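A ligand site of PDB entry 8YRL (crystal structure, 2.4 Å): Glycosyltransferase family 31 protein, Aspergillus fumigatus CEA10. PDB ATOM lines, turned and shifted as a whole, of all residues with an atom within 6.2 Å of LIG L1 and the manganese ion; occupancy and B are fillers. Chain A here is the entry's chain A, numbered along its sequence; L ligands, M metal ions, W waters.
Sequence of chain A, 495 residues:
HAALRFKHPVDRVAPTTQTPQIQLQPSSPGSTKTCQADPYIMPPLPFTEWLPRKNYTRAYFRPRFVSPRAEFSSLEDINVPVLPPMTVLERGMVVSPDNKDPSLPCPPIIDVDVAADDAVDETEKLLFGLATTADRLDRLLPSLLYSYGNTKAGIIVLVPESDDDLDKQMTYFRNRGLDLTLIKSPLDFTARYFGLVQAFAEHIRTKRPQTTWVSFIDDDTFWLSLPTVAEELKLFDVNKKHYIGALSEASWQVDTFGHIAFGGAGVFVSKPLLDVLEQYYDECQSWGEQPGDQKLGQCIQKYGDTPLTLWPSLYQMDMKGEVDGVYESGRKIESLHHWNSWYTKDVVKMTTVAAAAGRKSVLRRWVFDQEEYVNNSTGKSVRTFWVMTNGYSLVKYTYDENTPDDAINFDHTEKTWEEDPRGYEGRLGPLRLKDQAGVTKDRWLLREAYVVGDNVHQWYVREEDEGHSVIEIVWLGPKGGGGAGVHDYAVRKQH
N2 of LIG L1 lies within hydrogen-bond range of O of Ala 131, at 2.7 Å.
An oxygen (O4) of LG2 L2 lies within hydrogen-bond range of the side-chain carboxylate (OD2) of Asp 318, at 2.7 Å.
The side-chain hydroxyl (OG) of Ser 341 is in hydrogen-bond range of an oxygen (O8) of LIG L1, at 3.2 Å.
A ring nitrogen (NE2) of His 338 sits at hydrogen-bond distance from an oxygen (O11) of LIG L1 (2.6 Å).
NH2 of Arg 136 lies within hydrogen-bond range of O4 of LIG L1.
The side-chain carboxylate (OD2) of Asp 219 sits close to a nitrogen (N2) of LIG L1 (3.5 Å).
O2 of LIG L1 lies within hydrogen-bond range of N of Asp 219, at 2.8 Å.
O11 of LIG L1 is in hydrogen-bond range of O5 of LG2 L2, 2.5 Å away.
N of Asp 218 lies within hydrogen-bond range of OG1 of Thr 221 (3.2 Å).
OD2 of Asp 219 lies within salt-bridge range of NE of Arg 136.
A ring nitrogen (ND1) of His 338 lies within hydrogen-bond range of the backbone carbonyl oxygen of Gln 316, at 3.4 Å.
The side-chain carboxylate (OD2) of Asp 219 lies within hydrogen-bond range of the side-chain hydroxyl (OG1) of Thr 132, 3.0 Å away.
O of Thr 132 lies within hydrogen-bond range of NH2 of Arg 192 (3.1 Å).
The side-chain carboxylate of Asp 220 is in hydrogen-bond range of the backbone NH of His 338, at 3.3 Å.
N of Arg 136 lies within hydrogen-bond range of OG1 of Thr 133 (3.2 Å).
The side-chain hydroxyl of Thr 132 lies close to the guanidinium group of Arg 136.
Residues that only touch LIG L1: Thr 132 (3.5 Å), Phe 189 (3.2 Å) and Trp 342 (3.8 Å).
Hydrophobic or aromatic side chains that line LIG L1: Phe 189, His 337 and His 338.
The nearest printed residue that does not touch the manganese ion is His 338 (4.5 Å).
The manganese ion is bound by an oxygen (O7) of LIG L1 (1.9 Å), a ring nitrogen (NE2) of His 337 (2.1 Å), the side-chain carboxylate of Asp 218 (2.2 Å), the side-chain carboxylate of Asp 220 (2.4 Å) and an oxygen (O12) of LIG L1 (2.5 Å).
Water W7 bridges O11 of LIG L1 and NE1 of Trp 342.
Water W6 bridges NE2 of Gln 316 and N of Gly 264.
Water W2 lies within hydrogen-bond range of the backbone NH of Ala 131, an oxygen (O2) of LIG L1 and the backbone carbonyl oxygen of Ile 217.
Water W4 lies within hydrogen-bond range of the guanidinium group of Arg 136 and an oxygen (O8) of LIG L1.
Water W1 bridges OD1 of Asp 219 (2.6 Å) and NH2 of Arg 136 (2.7 Å).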
ATOM      1  N   LEU A 130      20.072  11.010  18.852  1.00  0.00           N
ATOM      2  CA  LEU A 130      19.249  10.360  17.855  1.00  0.00           C
ATOM      3  C   LEU A 130      19.209  11.193  16.584  1.00  0.00           C
ATOM      4  O   LEU A 130      19.151  12.427  16.638  1.00  0.00           O
ATOM      5  CB  LEU A 130      17.825  10.131  18.374  1.00  0.00           C
ATOM      6  CG  LEU A 130      17.608   8.922  19.277  1.00  0.00           C
ATOM      7  CD1 LEU A 130      16.266   9.000  19.988  1.00  0.00           C
ATOM      8  CD2 LEU A 130      17.705   7.647  18.473  1.00  0.00           C
ATOM      9  N   ALA A 131      19.234  10.512  15.442  1.00  0.00           N
ATOM     10  CA  ALA A 131      19.001  11.123  14.135  1.00  0.00           C
ATOM     11  C   ALA A 131      17.723  10.498  13.586  1.00  0.00           C
ATOM     12  O   ALA A 131      17.764   9.413  12.995  1.00  0.00           O
ATOM     13  CB  ALA A 131      20.192  10.903  13.202  1.00  0.00           C
ATOM     14  N   THR A 132      16.604  11.170  13.803  1.00  0.00           N
ATOM     15  CA  THR A 132      15.294  10.651  13.419  1.00  0.00           C
ATOM     16  C   THR A 132      14.330  11.819  13.306  1.00  0.00           C
ATOM     17  O   THR A 132      14.738  12.989  13.315  1.00  0.00           O
ATOM     18  CB  THR A 132      14.817   9.594  14.418  1.00  0.00           C
ATOM     19  OG1 THR A 132      13.611   8.981  13.938  1.00  0.00           O
ATOM     20  CG2 THR A 132      14.558  10.217  15.782  1.00  0.00           C
ATOM     21  N   THR A 133      13.040  11.513  13.197  1.00  0.00           N
ATOM     22  CA  THR A 133      12.003  12.521  13.067  1.00  0.00           C
ATOM     23  C   THR A 133      11.036  12.426  14.252  1.00  0.00           C
ATOM     24  O   THR A 133      11.002  11.430  14.971  1.00  0.00           O
ATOM     25  CB  THR A 133      11.223  12.372  11.757  1.00  0.00           C
ATOM     26  OG1 THR A 133      10.513  11.122  11.762  1.00  0.00           O
ATOM     27  CG2 THR A 133      12.179  12.396  10.568  1.00  0.00           C
ATOM     28  N   ARG A 136       8.656   9.490  13.785  1.00  0.00           N
ATOM     29  CA  ARG A 136       9.183   8.189  14.188  1.00  0.00           C
ATOM     30  C   ARG A 136       9.244   8.059  15.703  1.00  0.00           C
ATOM     31  O   ARG A 136       9.032   6.972  16.253  1.00  0.00           O
ATOM     32  CB  ARG A 136      10.572   7.966  13.577  1.00  0.00           C
ATOM     33  CG  ARG A 136      10.568   7.815  12.059  1.00  0.00           C
ATOM     34  CD  ARG A 136      11.970   7.559  11.533  1.00  0.00           C
ATOM     35  NE  ARG A 136      12.536   6.329  12.078  1.00  0.00           N
ATOM     36  CZ  ARG A 136      12.355   5.129  11.543  1.00  0.00           C
ATOM     37  NH1 ARG A 136      11.641   4.952  10.443  1.00  0.00           N
ATOM     38  NH2 ARG A 136      12.910   4.065  12.132  1.00  0.00           N
ATOM     39  N   PHE A 189      20.123  12.002   6.948  1.00  0.00           N
ATOM     40  CA  PHE A 189      20.095  11.049   8.061  1.00  0.00           C
ATOM     41  C   PHE A 189      21.462  10.426   8.309  1.00  0.00           C
ATOM     42  O   PHE A 189      21.864  10.226   9.459  1.00  0.00           O
ATOM     43  CB  PHE A 189      19.044   9.971   7.807  1.00  0.00           C
ATOM     44  CG  PHE A 189      19.232   8.748   8.663  1.00  0.00           C
ATOM     45  CD1 PHE A 189      18.842   8.756   9.994  1.00  0.00           C
ATOM     46  CD2 PHE A 189      19.787   7.594   8.139  1.00  0.00           C
ATOM     47  CE1 PHE A 189      19.012   7.643  10.786  1.00  0.00           C
ATOM     48  CE2 PHE A 189      19.957   6.470   8.929  1.00  0.00           C
ATOM     49  CZ  PHE A 189      19.570   6.500  10.254  1.00  0.00           C
ATOM     50  N   ARG A 192      23.607  13.263   9.694  1.00  0.00           N
ATOM     51  CA  ARG A 192      23.105  13.720  10.982  1.00  0.00           C
ATOM     52  C   ARG A 192      23.517  12.785  12.108  1.00  0.00           C
ATOM     53  O   ARG A 192      23.662  13.216  13.258  1.00  0.00           O
ATOM     54  CB  ARG A 192      21.584  13.864  10.939  1.00  0.00           C
ATOM     55  CG  ARG A 192      21.108  15.292  10.711  1.00  0.00           C
ATOM     56  CD  ARG A 192      19.676  15.335  10.203  1.00  0.00           C
ATOM     57  NE  ARG A 192      18.784  14.474  10.974  1.00  0.00           N
ATOM     58  CZ  ARG A 192      17.818  13.745  10.429  1.00  0.00           C
ATOM     59  NH1 ARG A 192      17.598  13.739   9.127  1.00  0.00           N
ATOM     60  NH2 ARG A 192      17.047  13.004  11.228  1.00  0.00           N
ATOM     61  N   ILE A 217      22.591   6.075  19.314  1.00  0.00           N
ATOM     62  CA  ILE A 217      21.544   5.067  19.338  1.00  0.00           C
ATOM     63  C   ILE A 217      20.646   5.236  18.123  1.00  0.00           C
ATOM     64  O   ILE A 217      20.530   6.309  17.545  1.00  0.00           O
ATOM     65  CB  ILE A 217      20.697   5.133  20.620  1.00  0.00           C
ATOM     66  CG1 ILE A 217      20.335   6.585  20.935  1.00  0.00           C
ATOM     67  CG2 ILE A 217      21.419   4.473  21.785  1.00  0.00           C
ATOM     68  CD1 ILE A 217      19.155   6.737  21.862  1.00  0.00           C
ATOM     69  N   ASP A 218      20.007   4.126  17.736  1.00  0.00           N
ATOM     70  CA  ASP A 218      18.893   4.147  16.808  1.00  0.00           C
ATOM     71  C   ASP A 218      17.596   4.338  17.584  1.00  0.00           C
ATOM     72  O   ASP A 218      17.518   4.100  18.780  1.00  0.00           O
ATOM     73  CB  ASP A 218      18.835   2.850  15.991  1.00  0.00           C
ATOM     74  CG  ASP A 218      19.794   2.851  14.822  1.00  0.00           C
ATOM     75  OD1 ASP A 218      20.859   3.499  14.908  1.00  0.00           O
ATOM     76  OD2 ASP A 218      19.483   2.195  13.805  1.00  0.00           O
ATOM     77  N   ASP A 219      16.551   4.785  16.863  1.00  0.00           N
ATOM     78  CA  ASP A 219      15.258   4.931  17.527  1.00  0.00           C
ATOM     79  C   ASP A 219      14.625   3.584  17.863  1.00  0.00           C
ATOM     80  O   ASP A 219      13.668   3.559  18.645  1.00  0.00           O
ATOM     81  CB  ASP A 219      14.304   5.765  16.662  1.00  0.00           C
ATOM     82  CG  ASP A 219      14.171   5.243  15.246  1.00  0.00           C
ATOM     83  OD1 ASP A 219      14.555   4.086  14.983  1.00  0.00           O
ATOM     84  OD2 ASP A 219      13.664   5.994  14.391  1.00  0.00           O
ATOM     85  N   ASP A 220      15.132   2.485  17.299  1.00  0.00           N
ATOM     86  CA  ASP A 220      14.691   1.149  17.658  1.00  0.00           C
ATOM     87  C   ASP A 220      15.727   0.394  18.478  1.00  0.00           C
ATOM     88  O   ASP A 220      15.696  -0.838  18.533  1.00  0.00           O
ATOM     89  CB  ASP A 220      14.317   0.354  16.407  1.00  0.00           C
ATOM     90  CG  ASP A 220      15.493   0.121  15.488  1.00  0.00           C
ATOM     91  OD1 ASP A 220      16.417   0.953  15.469  1.00  0.00           O
ATOM     92  OD2 ASP A 220      15.492  -0.907  14.774  1.00  0.00           O
ATOM     93  N   THR A 221      16.661   1.110  19.117  1.00  0.00           N
ATOM     94  CA  THR A 221      17.569   0.504  20.076  1.00  0.00           C
ATOM     95  C   THR A 221      16.836   0.402  21.413  1.00  0.00           C
ATOM     96  O   THR A 221      16.546   1.425  22.049  1.00  0.00           O
ATOM     97  CB  THR A 221      18.854   1.321  20.210  1.00  0.00           C
ATOM     98  OG1 THR A 221      19.587   1.264  18.987  1.00  0.00           O
ATOM     99  CG2 THR A 221      19.720   0.761  21.332  1.00  0.00           C
ATOM    100  N   GLY A 264      23.065  -0.068  15.848  1.00  0.00           N
ATOM    101  CA  GLY A 264      21.788  -0.615  16.282  1.00  0.00           C
ATOM    102  C   GLY A 264      21.816  -1.137  17.704  1.00  0.00           C
ATOM    103  O   GLY A 264      20.861  -0.966  18.464  1.00  0.00           O
ATOM    104  N   GLN A 316      22.914  -6.270  17.922  1.00  0.00           N
ATOM    105  CA  GLN A 316      22.472  -5.550  16.743  1.00  0.00           C
ATOM    106  C   GLN A 316      21.312  -6.243  16.053  1.00  0.00           C
ATOM    107  O   GLN A 316      20.452  -5.579  15.460  1.00  0.00           O
ATOM    108  CB  GLN A 316      23.651  -5.383  15.780  1.00  0.00           C
ATOM    109  CG  GLN A 316      23.264  -5.079  14.342  1.00  0.00           C
ATOM    110  CD  GLN A 316      22.967  -3.607  14.117  1.00  0.00           C
ATOM    111  OE1 GLN A 316      23.528  -2.742  14.781  1.00  0.00           O
ATOM    112  NE2 GLN A 316      22.066  -3.327  13.173  1.00  0.00           N
ATOM    113  N   ASP A 318      21.347  -8.426  13.370  1.00  0.00           N
ATOM    114  CA  ASP A 318      21.465  -8.431  11.906  1.00  0.00           C
ATOM    115  C   ASP A 318      20.994  -9.779  11.378  1.00  0.00           C
ATOM    116  O   ASP A 318      21.753 -10.593  10.837  1.00  0.00           O
ATOM    117  CB  ASP A 318      22.890  -8.125  11.484  1.00  0.00           C
ATOM    118  CG  ASP A 318      23.162  -6.635  11.358  1.00  0.00           C
ATOM    119  OD1 ASP A 318      22.181  -5.859  11.296  1.00  0.00           O
ATOM    120  OD2 ASP A 318      24.336  -6.238  11.314  1.00  0.00           O
ATOM    121  N   HIS A 337      17.406  -4.782  18.939  1.00  0.00           N
ATOM    122  CA  HIS A 337      17.386  -3.959  17.737  1.00  0.00           C
ATOM    123  C   HIS A 337      16.659  -4.712  16.629  1.00  0.00           C
ATOM    124  O   HIS A 337      16.496  -5.940  16.704  1.00  0.00           O
ATOM    125  CB  HIS A 337      18.812  -3.582  17.316  1.00  0.00           C
ATOM    126  CG  HIS A 337      18.874  -2.633  16.161  1.00  0.00           C
ATOM    127  ND1 HIS A 337      19.496  -2.949  14.967  1.00  0.00           N
ATOM    128  CD2 HIS A 337      18.398  -1.368  16.014  1.00  0.00           C
ATOM    129  CE1 HIS A 337      19.400  -1.919  14.134  1.00  0.00           C
ATOM    130  NE2 HIS A 337      18.738  -0.952  14.743  1.00  0.00           N
ATOM    131  N   HIS A 338      16.226  -3.966  15.616  1.00  0.00           N
ATOM    132  CA  HIS A 338      15.618  -4.477  14.393  1.00  0.00           C
ATOM    133  C   HIS A 338      14.269  -5.158  14.622  1.00  0.00           C
ATOM    134  O   HIS A 338      13.751  -5.815  13.717  1.00  0.00           O
ATOM    135  CB  HIS A 338      16.543  -5.451  13.659  1.00  0.00           C
ATOM    136  CG  HIS A 338      17.537  -4.781  12.754  1.00  0.00           C
ATOM    137  ND1 HIS A 338      18.768  -5.328  12.467  1.00  0.00           N
ATOM    138  CD2 HIS A 338      17.476  -3.612  12.082  1.00  0.00           C
ATOM    139  CE1 HIS A 338      19.421  -4.526  11.648  1.00  0.00           C
ATOM    140  NE2 HIS A 338      18.665  -3.476  11.406  1.00  0.00           N
ATOM    141  N   ASN A 340      11.340  -4.011  14.771  1.00  0.00           N
ATOM    142  CA  ASN A 340      10.219  -3.407  14.070  1.00  0.00           C
ATOM    143  C   ASN A 340      10.557  -3.154  12.602  1.00  0.00           C
ATOM    144  O   ASN A 340      10.036  -2.217  11.995  1.00  0.00           O
ATOM    145  CB  ASN A 340       9.780  -2.113  14.762  1.00  0.00           C
ATOM    146  CG  ASN A 340       8.328  -1.758  14.465  1.00  0.00           C
ATOM    147  OD1 ASN A 340       7.981  -0.584  14.337  1.00  0.00           O
ATOM    148  ND2 ASN A 340       7.478  -2.770  14.342  1.00  0.00           N
ATOM    149  N   SER A 341      11.434  -3.979  12.024  1.00  0.00           N
ATOM    150  CA  SER A 341      11.865  -3.798  10.651  1.00  0.00           C
ATOM    151  C   SER A 341      12.369  -5.103  10.044  1.00  0.00           C
ATOM    152  O   SER A 341      11.646  -5.756   9.283  1.00  0.00           O
ATOM    153  CB  SER A 341      12.955  -2.721  10.566  1.00  0.00           C
ATOM    154  OG  SER A 341      14.116  -3.140  11.256  1.00  0.00           O
ATOM    155  N   TRP A 342      13.607  -5.489  10.380  1.00  0.00           N
ATOM    156  CA  TRP A 342      14.154  -6.737   9.871  1.00  0.00           C
ATOM    157  C   TRP A 342      13.325  -7.935  10.334  1.00  0.00           C
ATOM    158  O   TRP A 342      13.101  -8.879   9.569  1.00  0.00           O
ATOM    159  CB  TRP A 342      15.608  -6.890  10.306  1.00  0.00           C
ATOM    160  CG  TRP A 342      16.571  -6.099   9.473  1.00  0.00           C
ATOM    161  CD1 TRP A 342      16.357  -4.870   8.918  1.00  0.00           C
ATOM    162  CD2 TRP A 342      17.894  -6.488   9.081  1.00  0.00           C
ATOM    163  NE1 TRP A 342      17.457  -4.469   8.210  1.00  0.00           N
ATOM    164  CE2 TRP A 342      18.418  -5.440   8.289  1.00  0.00           C
ATOM    165  CE3 TRP A 342      18.689  -7.608   9.325  1.00  0.00           C
ATOM    166  CZ2 TRP A 342      19.705  -5.493   7.744  1.00  0.00           C
ATOM    167  CZ3 TRP A 342      19.957  -7.661   8.774  1.00  0.00           C
ATOM    168  CH2 TRP A 342      20.452  -6.607   8.006  1.00  0.00           C
HETATM  169  N1  LIG L   1      16.072   5.658  10.842  1.00  0.00           N
HETATM  170  C1  LIG L   1      15.998   6.931  11.387  1.00  0.00           C
HETATM  171  N2  LIG L   1      16.469   7.036  12.671  1.00  0.00           N
HETATM  172  C2  LIG L   1      16.982   6.013  13.454  1.00  0.00           C
HETATM  173  C3  LIG L   1      17.012   4.732  12.819  1.00  0.00           C
HETATM  174  C4  LIG L   1      16.563   4.604  11.560  1.00  0.00           C
HETATM  175  O1  LIG L   1      15.565   7.892  10.770  1.00  0.00           O
HETATM  176  O2  LIG L   1      17.362   6.265  14.613  1.00  0.00           O
HETATM  177  C5  LIG L   1      15.587   5.486   9.468  1.00  0.00           C
HETATM  178  C6  LIG L   1      16.701   5.595   8.410  1.00  0.00           C
HETATM  179  O3  LIG L   1      16.205   6.203   7.227  1.00  0.00           O
HETATM  180  C7  LIG L   1      17.063   4.119   8.187  1.00  0.00           C
HETATM  181  C8  LIG L   1      15.704   3.443   8.318  1.00  0.00           C
HETATM  182  O4  LIG L   1      15.021   4.186   9.353  1.00  0.00           O
HETATM  183  O5  LIG L   1      17.622   3.896   6.901  1.00  0.00           O
HETATM  184  C9  LIG L   1      15.754   1.975   8.684  1.00  0.00           C
HETATM  185  O6  LIG L   1      16.462   1.817   9.933  1.00  0.00           O
HETATM  186  P1  LIG L   1      16.284   0.513  10.802  1.00  0.00           P
HETATM  187  O7  LIG L   1      16.652   0.862  12.196  1.00  0.00           O
HETATM  188  O8  LIG L   1      14.916  -0.112  10.585  1.00  0.00           O
HETATM  189  O9  LIG L   1      17.340  -0.519  10.210  1.00  0.00           O
HETATM  190  P2  LIG L   1      18.910  -0.266  10.170  1.00  0.00           P
HETATM  191  O10 LIG L   1      19.274   0.856   9.261  1.00  0.00           O
HETATM  192  O11 LIG L   1      19.459  -1.626   9.741  1.00  0.00           O
HETATM  193  O12 LIG L   1      19.247  -0.020  11.645  1.00  0.00           O
HETATM  194  C1  LG2 L   2      26.555  -0.071   8.823  1.00  0.00           C
HETATM  195  C2  LG2 L   2      25.763  -1.040   9.729  1.00  0.00           C
HETATM  196  C3  LG2 L   2      25.029  -2.030   8.784  1.00  0.00           C
HETATM  197  C4  LG2 L   2      23.949  -2.819   9.589  1.00  0.00           C
HETATM  198  C5  LG2 L   2      22.696  -2.672   8.677  1.00  0.00           C
HETATM  199  O1  LG2 L   2      27.647   0.384   9.539  1.00  0.00           O
HETATM  200  O2  LG2 L   2      24.781  -0.325  10.425  1.00  0.00           O
HETATM  201  O3  LG2 L   2      24.381  -1.326   7.747  1.00  0.00           O
HETATM  202  O4  LG2 L   2      24.376  -4.144   9.656  1.00  0.00           O
HETATM  203  C6  LG2 L   2      23.302  -2.120   7.345  1.00  0.00           C
HETATM  204  O5  LG2 L   2      21.923  -1.661   9.244  1.00  0.00           O
HETATM  205  O6  LG2 L   2      23.840  -3.180   6.659  1.00  0.00           O
HETATM  206 MN    MN M   1      17.924   0.617  13.643  1.00  0.00          MN
HETATM  207  O   HOH W   1      14.079   2.055  13.464  1.00  0.00           O
HETATM  208  O   HOH W   2      19.601   7.931  15.242  1.00  0.00           O
HETATM  209  O   HOH W   3      19.793   2.942  11.038  1.00  0.00           O
HETATM  210  O   HOH W   4      12.319   1.275  11.278  1.00  0.00           O
HETATM  211  O   HOH W   5      15.136  -1.635   7.907  1.00  0.00           O
HETATM  212  O   HOH W   6      21.935   0.015  12.568  1.00  0.00           O
HETATM  213  O   HOH W   7      18.874  -1.647   6.970  1.00  0.00           O
